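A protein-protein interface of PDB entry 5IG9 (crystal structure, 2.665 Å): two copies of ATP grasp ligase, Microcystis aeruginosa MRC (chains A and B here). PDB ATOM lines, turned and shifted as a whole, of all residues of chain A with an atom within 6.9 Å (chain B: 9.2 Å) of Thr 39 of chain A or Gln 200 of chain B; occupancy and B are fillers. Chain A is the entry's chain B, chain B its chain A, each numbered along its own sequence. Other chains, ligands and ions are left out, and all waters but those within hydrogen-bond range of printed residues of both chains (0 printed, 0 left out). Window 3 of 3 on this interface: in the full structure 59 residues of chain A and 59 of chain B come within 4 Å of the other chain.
The side-chain amide nitrogen of Asn 146 of chain B lies within hydrogen-bond range of the backbone carbonyl oxygen of Pro 38 of chain A (3.0 Å).
The side-chain amide nitrogen (ND2) of Asn 146 of chain B sits at hydrogen-bond distance from the backbone carbonyl oxygen (O) of Val 41 of chain A (2.9 Å).
The backbone NH (N) of Thr 39 of chain A sits at hydrogen-bond distance from the backbone carbonyl oxygen (O) of Gln 200 of chain B (3.2 Å).
The backbone carbonyl oxygen (O) of Pro 38 of chain A sits close to the backbone carbonyl oxygen (O) of Gln 200 of chain B.
Of the 13 printed residues of chain A, 6 touch a printed residue of chain B.
Hydrophobic or aromatic side chains of chain A within 4 Å of the printed part of chain B: Phe 37, Pro 38 and Leu 81.
Hydrophobic or aromatic side chains of chain B within 4 Å of the printed part of chain A: Pro 203.
Along chain B the printed residues that touch a printed residue of chain A span positions 146 to 203.
Among the printed residues, no Asp or Glu carboxylate lies within 4 Å of a Lys or Arg side-chain nitrogen of the other chain.
The backbone carbonyl oxygen (O) of Arg 36 of chain A is in hydrogen-bond range of the backbone NH (N) of Val 41 of chain A, at 2.8 Å.
The backbone NH of Gly 78 of chain A lies close to the backbone carbonyl oxygen of Phe 37 of chain A (3.4 Å).
Printed residues of chain B within 4 Å of Phe 37 of chain A: Asn 146 (3.4 Å) and Pro 203 (3.5 Å).
Printed residues of chain B within 4 Å of Pro 38 of chain A: Asn 146, Leu 199, Gln 200, Phe 201 and Cys 202.
Of the printed residues of chain B, Thr 39 of chain A touches Gln 200 (3.2 Å).
Of the printed residues of chain A, Leu 199 of chain B touches Pro 38.
Gln 200 of chain B touches just these residues of chain A: Pro 38 (3.1 Å) and Thr 39 (3.2 Å).
Printed residues of chain A within 4 Å of Pro 203 of chain B: Phe 37.
No position is printed for both chains.
Of the 11 pairs that touch across the chains among the printed residues, none has its exchanged pair printed and touching as well.
Among the printed residues, pairs that only touch across the chains: Phe 37 of chain A with Asn 146 of chain B, Phe 37 of chain A with Pro 203 of chain B, Pro 38 of chain A with Leu 199 of chain B, Pro 38 of chain A with Phe 201 of chain B, Pro 38 of chain A with Cys 202 of chain B, Lys 42 of chain A with Asn 146 of chain B and Leu 81 of chain A with Phe 201 of chain B.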
ATOM      1  N   ASP A  35      13.438  -3.754  -8.213  1.00  0.00           N
ATOM      2  CA  ASP A  35      13.772  -2.348  -8.027  1.00  0.00           C
ATOM      3  C   ASP A  35      15.179  -2.152  -7.482  1.00  0.00           C
ATOM      4  O   ASP A  35      15.766  -1.086  -7.689  1.00  0.00           O
ATOM      5  CB  ASP A  35      12.751  -1.677  -7.105  1.00  0.00           C
ATOM      6  CG  ASP A  35      12.679  -2.326  -5.736  1.00  0.00           C
ATOM      7  OD1 ASP A  35      12.909  -3.550  -5.640  1.00  0.00           O
ATOM      8  OD2 ASP A  35      12.391  -1.609  -4.753  1.00  0.00           O
ATOM      9  N   ARG A  36      15.739  -3.155  -6.807  1.00  0.00           N
ATOM     10  CA  ARG A  36      17.077  -3.057  -6.240  1.00  0.00           C
ATOM     11  C   ARG A  36      18.167  -3.454  -7.233  1.00  0.00           C
ATOM     12  O   ARG A  36      19.345  -3.493  -6.864  1.00  0.00           O
ATOM     13  CB  ARG A  36      17.163  -3.903  -4.965  1.00  0.00           C
ATOM     14  CG  ARG A  36      16.038  -3.589  -3.981  1.00  0.00           C
ATOM     15  CD  ARG A  36      16.413  -3.843  -2.526  1.00  0.00           C
ATOM     16  NE  ARG A  36      16.797  -5.229  -2.270  1.00  0.00           N
ATOM     17  CZ  ARG A  36      18.040  -5.620  -2.012  1.00  0.00           C
ATOM     18  NH1 ARG A  36      19.021  -4.729  -1.970  1.00  0.00           N
ATOM     19  NH2 ARG A  36      18.302  -6.901  -1.788  1.00  0.00           N
ATOM     20  N   PHE A  37      17.799  -3.745  -8.475  1.00  0.00           N
ATOM     21  CA  PHE A  37      18.753  -3.895  -9.566  1.00  0.00           C
ATOM     22  C   PHE A  37      18.669  -2.636 -10.420  1.00  0.00           C
ATOM     23  O   PHE A  37      17.574  -2.135 -10.662  1.00  0.00           O
ATOM     24  CB  PHE A  37      18.441  -5.153 -10.389  1.00  0.00           C
ATOM     25  CG  PHE A  37      19.063  -5.161 -11.762  1.00  0.00           C
ATOM     26  CD1 PHE A  37      20.356  -5.613 -11.950  1.00  0.00           C
ATOM     27  CD2 PHE A  37      18.340  -4.737 -12.870  1.00  0.00           C
ATOM     28  CE1 PHE A  37      20.927  -5.616 -13.204  1.00  0.00           C
ATOM     29  CE2 PHE A  37      18.907  -4.745 -14.130  1.00  0.00           C
ATOM     30  CZ  PHE A  37      20.202  -5.189 -14.296  1.00  0.00           C
ATOM     31  N   PRO A  38      19.813  -2.115 -10.891  1.00  0.00           N
ATOM     32  CA  PRO A  38      21.187  -2.602 -10.762  1.00  0.00           C
ATOM     33  C   PRO A  38      21.963  -1.997  -9.591  1.00  0.00           C
ATOM     34  O   PRO A  38      23.139  -2.312  -9.412  1.00  0.00           O
ATOM     35  CB  PRO A  38      21.810  -2.170 -12.086  1.00  0.00           C
ATOM     36  CG  PRO A  38      21.151  -0.855 -12.355  1.00  0.00           C
ATOM     37  CD  PRO A  38      19.741  -0.963 -11.808  1.00  0.00           C
ATOM     38  N   THR A  39      21.301  -1.142  -8.809  1.00  0.00           N
ATOM     39  CA  THR A  39      22.002  -0.400  -7.769  1.00  0.00           C
ATOM     40  C   THR A  39      22.524  -1.309  -6.666  1.00  0.00           C
ATOM     41  O   THR A  39      23.527  -0.983  -6.022  1.00  0.00           O
ATOM     42  CB  THR A  39      21.082   0.669  -7.180  1.00  0.00           C
ATOM     43  OG1 THR A  39      19.884   0.047  -6.702  1.00  0.00           O
ATOM     44  CG2 THR A  39      20.725   1.705  -8.236  1.00  0.00           C
ATOM     45  N   GLU A  40      21.873  -2.439  -6.432  1.00  0.00           N
ATOM     46  CA  GLU A  40      22.283  -3.289  -5.324  1.00  0.00           C
ATOM     47  C   GLU A  40      22.476  -4.738  -5.749  1.00  0.00           C
ATOM     48  O   GLU A  40      23.502  -5.348  -5.435  1.00  0.00           O
ATOM     49  CB  GLU A  40      21.254  -3.201  -4.189  1.00  0.00           C
ATOM     50  CG  GLU A  40      20.970  -1.781  -3.714  1.00  0.00           C
ATOM     51  CD  GLU A  40      19.920  -1.723  -2.615  1.00  0.00           C
ATOM     52  OE1 GLU A  40      20.001  -2.530  -1.667  1.00  0.00           O
ATOM     53  OE2 GLU A  40      19.005  -0.874  -2.706  1.00  0.00           O
ATOM     54  N   VAL A  41      21.503  -5.297  -6.456  1.00  0.00           N
ATOM     55  CA  VAL A  41      21.558  -6.698  -6.858  1.00  0.00           C
ATOM     56  C   VAL A  41      22.423  -6.838  -8.101  1.00  0.00           C
ATOM     57  O   VAL A  41      22.334  -6.029  -9.033  1.00  0.00           O
ATOM     58  CB  VAL A  41      20.140  -7.243  -7.103  1.00  0.00           C
ATOM     59  CG1 VAL A  41      20.189  -8.729  -7.405  1.00  0.00           C
ATOM     60  CG2 VAL A  41      19.253  -6.966  -5.900  1.00  0.00           C
ATOM     61  N   LYS A  42      23.271  -7.863  -8.112  1.00  0.00           N
ATOM     62  CA  LYS A  42      24.131  -8.172  -9.246  1.00  0.00           C
ATOM     63  C   LYS A  42      23.511  -9.299 -10.061  1.00  0.00           C
ATOM     64  O   LYS A  42      23.183 -10.357  -9.513  1.00  0.00           O
ATOM     65  CB  LYS A  42      25.531  -8.576  -8.779  1.00  0.00           C
ATOM     66  CG  LYS A  42      26.247  -7.540  -7.922  1.00  0.00           C
ATOM     67  CD  LYS A  42      26.515  -6.260  -8.696  1.00  0.00           C
ATOM     68  CE  LYS A  42      27.317  -5.273  -7.862  1.00  0.00           C
ATOM     69  NZ  LYS A  42      27.564  -3.996  -8.589  1.00  0.00           N
ATOM     70  N   GLY A  78      14.378  -1.367 -11.586  1.00  0.00           N
ATOM     71  CA  GLY A  78      15.280  -0.259 -11.352  1.00  0.00           C
ATOM     72  C   GLY A  78      14.644   1.024 -10.869  1.00  0.00           C
ATOM     73  O   GLY A  78      15.143   2.109 -11.186  1.00  0.00           O
ATOM     74  N   LYS A  80      14.706   2.035  -7.881  1.00  0.00           N
ATOM     75  CA  LYS A  80      15.550   2.553  -6.814  1.00  0.00           C
ATOM     76  C   LYS A  80      16.783   3.280  -7.341  1.00  0.00           C
ATOM     77  O   LYS A  80      17.732   3.501  -6.579  1.00  0.00           O
ATOM     78  CB  LYS A  80      15.967   1.424  -5.867  1.00  0.00           C
ATOM     79  CG  LYS A  80      14.955   1.120  -4.771  1.00  0.00           C
ATOM     80  CD  LYS A  80      15.552   1.375  -3.390  1.00  0.00           C
ATOM     81  CE  LYS A  80      14.539   1.137  -2.277  1.00  0.00           C
ATOM     82  NZ  LYS A  80      15.141   1.352  -0.930  1.00  0.00           N
ATOM     83  N   LEU A  81      16.798   3.634  -8.623  1.00  0.00           N
ATOM     84  CA  LEU A  81      17.823   4.535  -9.121  1.00  0.00           C
ATOM     85  C   LEU A  81      17.749   5.852  -8.354  1.00  0.00           C
ATOM     86  O   LEU A  81      16.652   6.315  -8.023  1.00  0.00           O
ATOM     87  CB  LEU A  81      17.643   4.803 -10.616  1.00  0.00           C
ATOM     88  CG  LEU A  81      17.805   3.671 -11.631  1.00  0.00           C
ATOM     89  CD1 LEU A  81      17.129   4.062 -12.937  1.00  0.00           C
ATOM     90  CD2 LEU A  81      19.270   3.349 -11.865  1.00  0.00           C
ATOM     91  N   PRO A  82      18.884   6.469  -8.042  1.00  0.00           N
ATOM     92  CA  PRO A  82      18.849   7.784  -7.386  1.00  0.00           C
ATOM     93  C   PRO A  82      18.143   8.815  -8.259  1.00  0.00           C
ATOM     94  O   PRO A  82      18.391   8.908  -9.464  1.00  0.00           O
ATOM     95  CB  PRO A  82      20.334   8.117  -7.194  1.00  0.00           C
ATOM     96  CG  PRO A  82      21.028   6.774  -7.205  1.00  0.00           C
ATOM     97  CD  PRO A  82      20.253   5.943  -8.178  1.00  0.00           C
ATOM     98  N   MET A  85      19.868  11.569 -10.426  1.00  0.00           N
ATOM     99  CA  MET A  85      20.449  11.242 -11.722  1.00  0.00           C
ATOM    100  C   MET A  85      19.807  12.074 -12.833  1.00  0.00           C
ATOM    101  O   MET A  85      18.663  12.524 -12.720  1.00  0.00           O
ATOM    102  CB  MET A  85      20.267   9.744 -12.025  1.00  0.00           C
ATOM    103  CG  MET A  85      21.024   9.193 -13.235  1.00  0.00           C
ATOM    104  SD  MET A  85      20.479   7.506 -13.596  1.00  0.00           S
ATOM    105  CE  MET A  85      20.610   6.760 -11.970  1.00  0.00           C
ATOM    106  N   SER B 145      25.419  -7.636 -18.040  1.00  0.00           N
ATOM    107  CA  SER B 145      25.843  -7.598 -16.649  1.00  0.00           C
ATOM    108  C   SER B 145      25.908  -6.165 -16.141  1.00  0.00           C
ATOM    109  O   SER B 145      26.194  -5.231 -16.895  1.00  0.00           O
ATOM    110  CB  SER B 145      27.209  -8.277 -16.481  1.00  0.00           C
ATOM    111  OG  SER B 145      27.686  -8.153 -15.154  1.00  0.00           O
ATOM    112  N   ASN B 146      25.630  -6.014 -14.844  1.00  0.00           N
ATOM    113  CA  ASN B 146      25.878  -4.791 -14.090  1.00  0.00           C
ATOM    114  C   ASN B 146      26.999  -4.983 -13.075  1.00  0.00           C
ATOM    115  O   ASN B 146      27.151  -4.174 -12.154  1.00  0.00           O
ATOM    116  CB  ASN B 146      24.601  -4.332 -13.382  1.00  0.00           C
ATOM    117  CG  ASN B 146      24.169  -5.285 -12.281  1.00  0.00           C
ATOM    118  OD1 ASN B 146      24.136  -6.499 -12.473  1.00  0.00           O
ATOM    119  ND2 ASN B 146      23.845  -4.735 -11.115  1.00  0.00           N
ATOM    120  N   ASN B 147      27.781  -6.045 -13.229  1.00  0.00           N
ATOM    121  CA  ASN B 147      28.775  -6.467 -12.244  1.00  0.00           C
ATOM    122  C   ASN B 147      30.174  -6.308 -12.821  1.00  0.00           C
ATOM    123  O   ASN B 147      30.545  -7.053 -13.749  1.00  0.00           O
ATOM    124  CB  ASN B 147      28.513  -7.918 -11.841  1.00  0.00           C
ATOM    125  CG  ASN B 147      29.546  -8.457 -10.876  1.00  0.00           C
ATOM    126  OD1 ASN B 147      30.270  -7.701 -10.236  1.00  0.00           O
ATOM    127  ND2 ASN B 147      29.614  -9.781 -10.763  1.00  0.00           N
ATOM    128  N   PRO B 148      30.983  -5.371 -12.317  1.00  0.00           N
ATOM    129  CA  PRO B 148      32.312  -5.153 -12.916  1.00  0.00           C
ATOM    130  C   PRO B 148      33.232  -6.364 -12.871  1.00  0.00           C
ATOM    131  O   PRO B 148      34.009  -6.560 -13.814  1.00  0.00           O
ATOM    132  CB  PRO B 148      32.878  -3.988 -12.091  1.00  0.00           C
ATOM    133  CG  PRO B 148      31.676  -3.268 -11.588  1.00  0.00           C
ATOM    134  CD  PRO B 148      30.649  -4.337 -11.324  1.00  0.00           C
ATOM    135  N   ASN B 195      36.896   2.101 -15.571  1.00  0.00           N
ATOM    136  CA  ASN B 195      35.783   2.983 -15.235  1.00  0.00           C
ATOM    137  C   ASN B 195      34.467   2.221 -15.304  1.00  0.00           C
ATOM    138  O   ASN B 195      33.476   2.682 -15.875  1.00  0.00           O
ATOM    139  CB  ASN B 195      35.762   4.193 -16.162  1.00  0.00           C
ATOM    140  CG  ASN B 195      37.093   4.911 -16.204  1.00  0.00           C
ATOM    141  OD1 ASN B 195      37.787   5.015 -15.192  1.00  0.00           O
ATOM    142  ND2 ASN B 195      37.466   5.401 -17.381  1.00  0.00           N
ATOM    143  N   LEU B 196      34.444   1.033 -14.706  1.00  0.00           N
ATOM    144  CA  LEU B 196      33.260   0.184 -14.712  1.00  0.00           C
ATOM    145  C   LEU B 196      32.286   0.504 -13.588  1.00  0.00           C
ATOM    146  O   LEU B 196      31.299  -0.223 -13.426  1.00  0.00           O
ATOM    147  CB  LEU B 196      33.665  -1.289 -14.616  1.00  0.00           C
ATOM    148  CG  LEU B 196      34.334  -1.960 -15.814  1.00  0.00           C
ATOM    149  CD1 LEU B 196      34.512  -3.436 -15.516  1.00  0.00           C
ATOM    150  CD2 LEU B 196      33.518  -1.763 -17.074  1.00  0.00           C
ATOM    151  N   GLU B 197      32.532   1.560 -12.810  1.00  0.00           N
ATOM    152  CA  GLU B 197      31.693   1.837 -11.651  1.00  0.00           C
ATOM    153  C   GLU B 197      30.288   2.284 -12.037  1.00  0.00           C
ATOM    154  O   GLU B 197      29.366   2.155 -11.225  1.00  0.00           O
ATOM    155  CB  GLU B 197      32.364   2.889 -10.768  1.00  0.00           C
ATOM    156  CG  GLU B 197      32.685   4.180 -11.495  1.00  0.00           C
ATOM    157  CD  GLU B 197      34.054   4.719 -11.142  1.00  0.00           C
ATOM    158  OE1 GLU B 197      34.793   5.113 -12.069  1.00  0.00           O
ATOM    159  OE2 GLU B 197      34.393   4.741  -9.940  1.00  0.00           O
ATOM    160  N   GLY B 198      30.099   2.787 -13.256  1.00  0.00           N
ATOM    161  CA  GLY B 198      28.780   3.188 -13.704  1.00  0.00           C
ATOM    162  C   GLY B 198      27.828   2.051 -14.006  1.00  0.00           C
ATOM    163  O   GLY B 198      26.660   2.311 -14.310  1.00  0.00           O
ATOM    164  N   LEU B 199      28.291   0.799 -13.933  1.00  0.00           N
ATOM    165  CA  LEU B 199      27.421  -0.339 -14.206  1.00  0.00           C
ATOM    166  C   LEU B 199      26.339  -0.511 -13.151  1.00  0.00           C
ATOM    167  O   LEU B 199      25.301  -1.115 -13.442  1.00  0.00           O
ATOM    168  CB  LEU B 199      28.244  -1.624 -14.309  1.00  0.00           C
ATOM    169  CG  LEU B 199      28.892  -1.913 -15.663  1.00  0.00           C
ATOM    170  CD1 LEU B 199      29.687  -3.208 -15.609  1.00  0.00           C
ATOM    171  CD2 LEU B 199      27.833  -1.974 -16.750  1.00  0.00           C
ATOM    172  N   GLN B 200      26.554   0.005 -11.939  1.00  0.00           N
ATOM    173  CA  GLN B 200      25.542  -0.090 -10.894  1.00  0.00           C
ATOM    174  C   GLN B 200      24.318   0.766 -11.184  1.00  0.00           C
ATOM    175  O   GLN B 200      23.320   0.646 -10.467  1.00  0.00           O
ATOM    176  CB  GLN B 200      26.135   0.312  -9.542  1.00  0.00           C
ATOM    177  CG  GLN B 200      26.493   1.785  -9.432  1.00  0.00           C
ATOM    178  CD  GLN B 200      27.050   2.149  -8.066  1.00  0.00           C
ATOM    179  OE1 GLN B 200      26.544   1.701  -7.035  1.00  0.00           O
ATOM    180  NE2 GLN B 200      28.107   2.956  -8.054  1.00  0.00           N
ATOM    181  N   PHE B 201      24.367   1.623 -12.203  1.00  0.00           N
ATOM    182  CA  PHE B 201      23.231   2.452 -12.574  1.00  0.00           C
ATOM    183  C   PHE B 201      22.568   2.018 -13.872  1.00  0.00           C
ATOM    184  O   PHE B 201      21.444   2.452 -14.147  1.00  0.00           O
ATOM    185  CB  PHE B 201      23.658   3.922 -12.688  1.00  0.00           C
ATOM    186  CG  PHE B 201      24.388   4.433 -11.478  1.00  0.00           C
ATOM    187  CD1 PHE B 201      23.772   4.446 -10.238  1.00  0.00           C
ATOM    188  CD2 PHE B 201      25.688   4.902 -11.582  1.00  0.00           C
ATOM    189  CE1 PHE B 201      24.439   4.912  -9.121  1.00  0.00           C
ATOM    190  CE2 PHE B 201      26.361   5.371 -10.467  1.00  0.00           C
ATOM    191  CZ  PHE B 201      25.735   5.377  -9.236  1.00  0.00           C
ATOM    192  N   CYS B 202      23.229   1.179 -14.669  1.00  0.00           N
ATOM    193  CA  CYS B 202      22.695   0.670 -15.926  1.00  0.00           C
ATOM    194  C   CYS B 202      23.591  -0.440 -16.458  1.00  0.00           C
ATOM    195  O   CYS B 202      24.779  -0.206 -16.723  1.00  0.00           O
ATOM    196  CB  CYS B 202      22.573   1.784 -16.965  1.00  0.00           C
ATOM    197  SG  CYS B 202      21.822   1.243 -18.515  1.00  0.00           S
ATOM    198  N   PRO B 203      23.072  -1.653 -16.623  1.00  0.00           N
ATOM    199  CA  PRO B 203      23.880  -2.731 -17.200  1.00  0.00           C
ATOM    200  C   PRO B 203      24.125  -2.493 -18.681  1.00  0.00           C
ATOM    201  O   PRO B 203      23.538  -1.616 -19.316  1.00  0.00           O
ATOM    202  CB  PRO B 203      23.027  -3.980 -16.971  1.00  0.00           C
ATOM    203  CG  PRO B 203      21.634  -3.463 -16.934  1.00  0.00           C
ATOM    204  CD  PRO B 203      21.719  -2.110 -16.272  1.00  0.00           C
ATOM    205  N   MET B 204      25.029  -3.297 -19.230  1.00  0.00           N
ATOM    206  CA  MET B 204      25.272  -3.316 -20.663  1.00  0.00           C
ATOM    207  C   MET B 204      25.410  -4.760 -21.111  1.00  0.00           C
ATOM    208  O   MET B 204      25.510  -5.680 -20.295  1.00  0.00           O
ATOM    209  CB  MET B 204      26.514  -2.508 -21.049  1.00  0.00           C
ATOM    210  CG  MET B 204      26.413  -1.034 -20.725  1.00  0.00           C
ATOM    211  SD  MET B 204      27.561  -0.029 -21.679  1.00  0.00           S
ATOM    212  CE  MET B 204      26.858  -0.191 -23.317  1.00  0.00           C
